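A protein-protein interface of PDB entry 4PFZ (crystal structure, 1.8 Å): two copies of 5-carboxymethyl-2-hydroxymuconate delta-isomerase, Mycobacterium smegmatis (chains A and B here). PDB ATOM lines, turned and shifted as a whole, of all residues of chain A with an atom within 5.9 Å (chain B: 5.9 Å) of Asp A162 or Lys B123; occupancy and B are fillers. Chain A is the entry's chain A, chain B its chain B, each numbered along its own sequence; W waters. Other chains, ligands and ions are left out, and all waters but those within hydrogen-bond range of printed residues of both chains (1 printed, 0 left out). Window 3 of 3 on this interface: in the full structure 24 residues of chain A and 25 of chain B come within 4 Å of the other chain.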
ATOM      1  N   THR A  90       7.187  26.611 -12.118  1.00  0.00           N
ATOM      2  CA  THR A  90       7.039  26.532 -10.667  1.00  0.00           C
ATOM      3  C   THR A  90       6.088  25.408 -10.223  1.00  0.00           C
ATOM      4  O   THR A  90       5.991  25.099  -9.028  1.00  0.00           O
ATOM      5  CB  THR A  90       6.528  27.883 -10.097  1.00  0.00           C
ATOM      6  OG1 THR A  90       5.468  28.375 -10.923  1.00  0.00           O
ATOM      7  CG2 THR A  90       7.654  28.897 -10.099  1.00  0.00           C
ATOM      8  N   ALA A  91       5.409  24.793 -11.192  1.00  0.00           N
ATOM      9  CA  ALA A  91       4.510  23.674 -10.945  1.00  0.00           C
ATOM     10  C   ALA A  91       5.260  22.354 -10.933  1.00  0.00           C
ATOM     11  O   ALA A  91       4.749  21.366 -10.424  1.00  0.00           O
ATOM     12  CB  ALA A  91       3.411  23.634 -12.002  1.00  0.00           C
ATOM     13  N   ILE A  93       7.448  19.292  -9.979  1.00  0.00           N
ATOM     14  CA  ILE A  93       8.038  18.577  -8.846  1.00  0.00           C
ATOM     15  C   ILE A  93       8.571  17.260  -9.387  1.00  0.00           C
ATOM     16  O   ILE A  93       8.193  16.855 -10.477  1.00  0.00           O
ATOM     17  CB  ILE A  93       7.042  18.277  -7.713  1.00  0.00           C
ATOM     18  CG1 ILE A  93       5.799  17.593  -8.280  1.00  0.00           C
ATOM     19  CG2 ILE A  93       6.669  19.548  -6.923  1.00  0.00           C
ATOM     20  CD1 ILE A  93       4.789  17.099  -7.195  1.00  0.00           C
ATOM     21  N   GLN A 100       0.101  18.726  -3.993  1.00  0.00           N
ATOM     22  CA  GLN A 100      -0.661  19.409  -2.956  1.00  0.00           C
ATOM     23  C   GLN A 100      -1.909  20.016  -3.542  1.00  0.00           C
ATOM     24  O   GLN A 100      -1.834  20.935  -4.359  1.00  0.00           O
ATOM     25  CB  GLN A 100       0.181  20.496  -2.283  1.00  0.00           C
ATOM     26  CG  GLN A 100       1.461  19.964  -1.651  1.00  0.00           C
ATOM     27  CD  GLN A 100       2.171  21.004  -0.804  1.00  0.00           C
ATOM     28  OE1 GLN A 100       1.560  21.653   0.051  1.00  0.00           O
ATOM     29  NE2 GLN A 100       3.464  21.175  -1.040  1.00  0.00           N
ATOM     30  N   GLY A 160      -1.825  25.219 -13.197  1.00  0.00           N
ATOM     31  CA  GLY A 160      -0.597  25.951 -12.906  1.00  0.00           C
ATOM     32  C   GLY A 160      -0.240  26.085 -11.434  1.00  0.00           C
ATOM     33  O   GLY A 160       0.717  26.778 -11.081  1.00  0.00           O
ATOM     34  N   HIS A 161      -0.996  25.415 -10.567  1.00  0.00           N
ATOM     35  CA  HIS A 161      -0.697  25.461  -9.138  1.00  0.00           C
ATOM     36  C   HIS A 161       0.659  24.839  -8.886  1.00  0.00           C
ATOM     37  O   HIS A 161       1.069  23.942  -9.621  1.00  0.00           O
ATOM     38  CB  HIS A 161      -1.776  24.736  -8.324  1.00  0.00           C
ATOM     39  CG  HIS A 161      -3.110  25.395  -8.408  1.00  0.00           C
ATOM     40  ND1 HIS A 161      -3.505  26.379  -7.525  1.00  0.00           N
ATOM     41  CD2 HIS A 161      -4.114  25.262  -9.301  1.00  0.00           C
ATOM     42  CE1 HIS A 161      -4.709  26.806  -7.859  1.00  0.00           C
ATOM     43  NE2 HIS A 161      -5.102  26.148  -8.935  1.00  0.00           N
ATOM     44  N   ASP A 162       1.348  25.301  -7.842  1.00  0.00           N
ATOM     45  CA  ASP A 162       2.550  24.615  -7.388  1.00  0.00           C
ATOM     46  C   ASP A 162       2.242  23.116  -7.234  1.00  0.00           C
ATOM     47  O   ASP A 162       1.158  22.743  -6.781  1.00  0.00           O
ATOM     48  CB  ASP A 162       3.061  25.211  -6.065  1.00  0.00           C
ATOM     49  CG  ASP A 162       3.764  26.574  -6.252  1.00  0.00           C
ATOM     50  OD1 ASP A 162       3.760  27.129  -7.381  1.00  0.00           O
ATOM     51  OD2 ASP A 162       4.324  27.091  -5.258  1.00  0.00           O
ATOM     52  N   THR A 163       3.196  22.293  -7.672  1.00  0.00           N
ATOM     53  CA  THR A 163       3.161  20.819  -7.651  1.00  0.00           C
ATOM     54  C   THR A 163       2.262  20.189  -8.712  1.00  0.00           C
ATOM     55  O   THR A 163       2.128  18.971  -8.720  1.00  0.00           O
ATOM     56  CB  THR A 163       2.733  20.212  -6.266  1.00  0.00           C
ATOM     57  OG1 THR A 163       1.304  20.275  -6.092  1.00  0.00           O
ATOM     58  CG2 THR A 163       3.460  20.861  -5.075  1.00  0.00           C
ATOM     59  N   PHE A 164       1.673  20.978  -9.623  1.00  0.00           N
ATOM     60  CA  PHE A 164       0.731  20.379 -10.575  1.00  0.00           C
ATOM     61  C   PHE A 164       1.432  19.894 -11.850  1.00  0.00           C
ATOM     62  O   PHE A 164       0.776  19.594 -12.836  1.00  0.00           O
ATOM     63  CB  PHE A 164      -0.407  21.339 -10.958  1.00  0.00           C
ATOM     64  CG  PHE A 164      -1.565  21.332  -9.995  1.00  0.00           C
ATOM     65  CD1 PHE A 164      -1.385  20.996  -8.655  1.00  0.00           C
ATOM     66  CD2 PHE A 164      -2.845  21.620 -10.439  1.00  0.00           C
ATOM     67  CE1 PHE A 164      -2.467  20.981  -7.774  1.00  0.00           C
ATOM     68  CE2 PHE A 164      -3.925  21.604  -9.567  1.00  0.00           C
ATOM     69  CZ  PHE A 164      -3.737  21.292  -8.228  1.00  0.00           C
ATOM     70  N   CYS A 165       2.757  19.818 -11.821  1.00  0.00           N
ATOM     71  CA  CYS A 165       3.491  19.210 -12.931  1.00  0.00           C
ATOM     72  C   CYS A 165       4.589  18.256 -12.458  1.00  0.00           C
ATOM     73  O   CYS A 165       5.781  18.534 -12.624  1.00  0.00           O
ATOM     74  CB  CYS A 165       4.097  20.301 -13.825  1.00  0.00           C
ATOM     75  SG  CYS A 165       4.642  19.682 -15.459  1.00  0.00           S
ATOM     76  N   LYS A 256      -4.402  20.485   0.961  1.00  0.00           N
ATOM     77  CA  LYS A 256      -4.039  21.576   1.865  1.00  0.00           C
ATOM     78  C   LYS A 256      -5.198  22.012   2.766  1.00  0.00           C
ATOM     79  O   LYS A 256      -6.352  21.623   2.556  1.00  0.00           O
ATOM     80  CB  LYS A 256      -3.527  22.775   1.063  1.00  0.00           C
ATOM     81  CG  LYS A 256      -2.306  22.467   0.230  1.00  0.00           C
ATOM     82  CD  LYS A 256      -1.888  23.673  -0.606  1.00  0.00           C
ATOM     83  CE  LYS A 256      -1.307  24.750   0.279  1.00  0.00           C
ATOM     84  NZ  LYS A 256      -0.372  24.163   1.279  1.00  0.00           N
ATOM     85  N   PRO B 121      10.658  36.496  -3.850  1.00  0.00           N
ATOM     86  CA  PRO B 121       9.908  35.242  -3.941  1.00  0.00           C
ATOM     87  C   PRO B 121       8.683  35.314  -3.054  1.00  0.00           C
ATOM     88  O   PRO B 121       8.784  35.810  -1.925  1.00  0.00           O
ATOM     89  CB  PRO B 121      10.908  34.187  -3.448  1.00  0.00           C
ATOM     90  CG  PRO B 121      11.942  34.937  -2.714  1.00  0.00           C
ATOM     91  CD  PRO B 121      12.004  36.309  -3.286  1.00  0.00           C
ATOM     92  N   CYS B 122       7.533  34.876  -3.554  1.00  0.00           N
ATOM     93  CA  CYS B 122       6.346  34.898  -2.722  1.00  0.00           C
ATOM     94  C   CYS B 122       5.252  33.946  -3.152  1.00  0.00           C
ATOM     95  O   CYS B 122       5.154  33.531  -4.310  1.00  0.00           O
ATOM     96  CB  CYS B 122       5.776  36.309  -2.656  1.00  0.00           C
ATOM     97  SG  CYS B 122       5.486  37.048  -4.251  1.00  0.00           S
ATOM     98  N   LYS B 123       4.421  33.626  -2.175  1.00  0.00           N
ATOM     99  CA  LYS B 123       3.307  32.716  -2.318  1.00  0.00           C
ATOM    100  C   LYS B 123       2.251  33.198  -1.339  1.00  0.00           C
ATOM    101  O   LYS B 123       2.597  33.639  -0.246  1.00  0.00           O
ATOM    102  CB  LYS B 123       3.746  31.276  -2.011  1.00  0.00           C
ATOM    103  CG  LYS B 123       2.705  30.208  -2.313  1.00  0.00           C
ATOM    104  CD  LYS B 123       2.525  30.043  -3.830  1.00  0.00           C
ATOM    105  CE  LYS B 123       1.378  29.096  -4.126  1.00  0.00           C
ATOM    106  NZ  LYS B 123       1.492  27.831  -3.324  1.00  0.00           N
ATOM    107  N   ASP B 124       0.980  33.148  -1.732  1.00  0.00           N
ATOM    108  CA  ASP B 124      -0.122  33.435  -0.810  1.00  0.00           C
ATOM    109  C   ASP B 124       0.010  34.809  -0.182  1.00  0.00           C
ATOM    110  O   ASP B 124      -0.051  34.950   1.041  1.00  0.00           O
ATOM    111  CB  ASP B 124      -0.188  32.384   0.308  1.00  0.00           C
ATOM    112  CG  ASP B 124      -0.467  30.991  -0.215  1.00  0.00           C
ATOM    113  OD1 ASP B 124      -1.314  30.866  -1.119  1.00  0.00           O
ATOM    114  OD2 ASP B 124       0.159  30.024   0.280  1.00  0.00           O
ATOM    115  N   VAL B 125       0.203  35.817  -1.017  1.00  0.00           N
ATOM    116  CA  VAL B 125       0.337  37.176  -0.521  1.00  0.00           C
ATOM    117  C   VAL B 125      -1.029  37.827  -0.427  1.00  0.00           C
ATOM    118  O   VAL B 125      -1.785  37.817  -1.395  1.00  0.00           O
ATOM    119  CB  VAL B 125       1.241  38.001  -1.439  1.00  0.00           C
ATOM    120  CG1 VAL B 125       1.352  39.435  -0.932  1.00  0.00           C
ATOM    121  CG2 VAL B 125       2.602  37.349  -1.524  1.00  0.00           C
ATOM    122  N   SER B 211      -0.382  34.937  -6.777  1.00  0.00           N
ATOM    123  CA  SER B 211       0.485  34.243  -5.827  1.00  0.00           C
ATOM    124  C   SER B 211      -0.257  33.187  -5.000  1.00  0.00           C
ATOM    125  O   SER B 211       0.385  32.392  -4.317  1.00  0.00           O
ATOM    126  CB  SER B 211       1.168  35.242  -4.891  1.00  0.00           C
ATOM    127  OG  SER B 211       0.224  35.926  -4.091  1.00  0.00           O
ATOM    128  N   ALA B 212      -1.592  33.179  -5.048  1.00  0.00           N
ATOM    129  CA  ALA B 212      -2.351  32.091  -4.424  1.00  0.00           C
ATOM    130  C   ALA B 212      -2.263  30.837  -5.295  1.00  0.00           C
ATOM    131  O   ALA B 212      -2.321  29.716  -4.801  1.00  0.00           O
ATOM    132  CB  ALA B 212      -3.826  32.497  -4.191  1.00  0.00           C
ATOM    133  N   VAL B 213      -2.118  31.051  -6.597  1.00  0.00           N
ATOM    134  CA  VAL B 213      -1.999  29.967  -7.558  1.00  0.00           C
ATOM    135  C   VAL B 213      -0.575  29.401  -7.643  1.00  0.00           C
ATOM    136  O   VAL B 213      -0.351  28.183  -7.560  1.00  0.00           O
ATOM    137  CB  VAL B 213      -2.424  30.435  -8.971  1.00  0.00           C
ATOM    138  CG1 VAL B 213      -2.236  29.314  -9.987  1.00  0.00           C
ATOM    139  CG2 VAL B 213      -3.870  30.940  -8.978  1.00  0.00           C
ATOM    140  N   MET B 214       0.390  30.294  -7.820  1.00  0.00           N
ATOM    141  CA  MET B 214       1.756  29.898  -8.151  1.00  0.00           C
ATOM    142  C   MET B 214       2.801  30.743  -7.430  1.00  0.00           C
ATOM    143  O   MET B 214       2.570  31.912  -7.131  1.00  0.00           O
ATOM    144  CB  MET B 214       1.977  29.994  -9.665  1.00  0.00           C
ATOM    145  CG  MET B 214       1.966  31.430 -10.188  1.00  0.00           C
ATOM    146  SD  MET B 214       2.087  31.436 -11.989  1.00  0.00           S
ATOM    147  CE  MET B 214       0.446  30.913 -12.449  1.00  0.00           C
ATOM    148  N   THR B 215       3.952  30.139  -7.159  1.00  0.00           N
ATOM    149  CA  THR B 215       5.076  30.848  -6.579  1.00  0.00           C
ATOM    150  C   THR B 215       5.561  31.909  -7.564  1.00  0.00           C
ATOM    151  O   THR B 215       5.800  31.615  -8.727  1.00  0.00           O
ATOM    152  CB  THR B 215       6.241  29.874  -6.211  1.00  0.00           C
ATOM    153  OG1 THR B 215       5.899  29.128  -5.033  1.00  0.00           O
ATOM    154  CG2 THR B 215       7.528  30.635  -5.947  1.00  0.00           C
ATOM    155  N   LEU B 216       5.670  33.152  -7.092  1.00  0.00           N
ATOM    156  CA  LEU B 216       6.215  34.231  -7.915  1.00  0.00           C
ATOM    157  C   LEU B 216       7.675  34.498  -7.555  1.00  0.00           C
ATOM    158  O   LEU B 216       8.024  34.583  -6.390  1.00  0.00           O
ATOM    159  CB  LEU B 216       5.386  35.508  -7.759  1.00  0.00           C
ATOM    160  CG  LEU B 216       3.935  35.431  -8.229  1.00  0.00           C
ATOM    161  CD1 LEU B 216       3.193  36.756  -7.981  1.00  0.00           C
ATOM    162  CD2 LEU B 216       3.900  35.098  -9.696  1.00  0.00           C
HETATM  163  O   HOH W   1       0.253  26.621  -5.421  1.00  0.00           O
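OD2 of Asp A162 lies within salt-bridge range of NZ of Lys B123 (3.5 Å). N of Asp A162 sits at hydrogen-bond distance from O of Val B213 (3.4 Å). The side-chain hydroxyl (OG1) of Thr B215 lies within hydrogen-bond range of the side-chain carboxylate (OD2) of Asp A162 (2.6 Å).
Among the printed residues, merely in contact across the chains: His A161 with Val B213 (3.2 Å), Asp A162 with Met B214 (3.5 Å), Thr A90 with Thr B215 (3.6 Å), Gly A160 with Met B214 (3.7 Å) and Gly A160 with Val B213 (3.9 Å).
Printed residues of chain B within 4 Å of Thr A90: Thr B215 (3.6 Å). Of the printed residues of chain B, Gly A160 touches Val B213 and Met B214. Of chain B, only Lys B123 (3.5 Å), Val B213 (3.4 Å), Met B214 (3.5 Å) and Thr B215 (2.6 Å) come within 4 Å of Asp A162. Lys B123 touches one residue of chain A. Of the printed residues of chain A, Val B213 touches Gly A160, His A161 and Asp A162. Of the printed residues of chain A, Met B214 touches Gly A160 (3.7 Å) and Asp A162 (3.5 Å). Printed residues of chain A within 4 Å of Thr B215: Thr A90 (3.6 Å) and Asp A162 (2.6 Å). The nearest printed residue of chain B that does not touch Asp A162 is Leu B216 (6.3 Å). The nearest residue of chain A that does not touch Lys B123 is Lys A256 (5.5 Å). The nearest printed residue of chain A that does not touch Met B214 is Thr A90 (4.05 Å).
Along chain A the printed residues that touch a printed residue of chain B span positions 90 to 162. Hydrophobic or aromatic side chains of chain B within 4 Å of the printed part of chain A: Met B214. Among the printed residues, 8 pairs touch across the chains. Among the printed residues, Asp or Glu carboxylates within 4 Å of a Lys or Arg side-chain nitrogen of the other chain: Asp A162 with Lys B123 (3.5 Å).
No position is printed for both chains. Of the 8 pairs that touch across the chains among the printed residues, none has its exchanged pair printed and touching as well.
Water W1 lies within hydrogen-bond range of the backbone carbonyl oxygen (O) of Val B213 (2.7 Å), the side-chain amino group (NZ) of Lys B123 (2.7 Å) and the backbone NH (N) of Asp A162 (3.0 Å).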
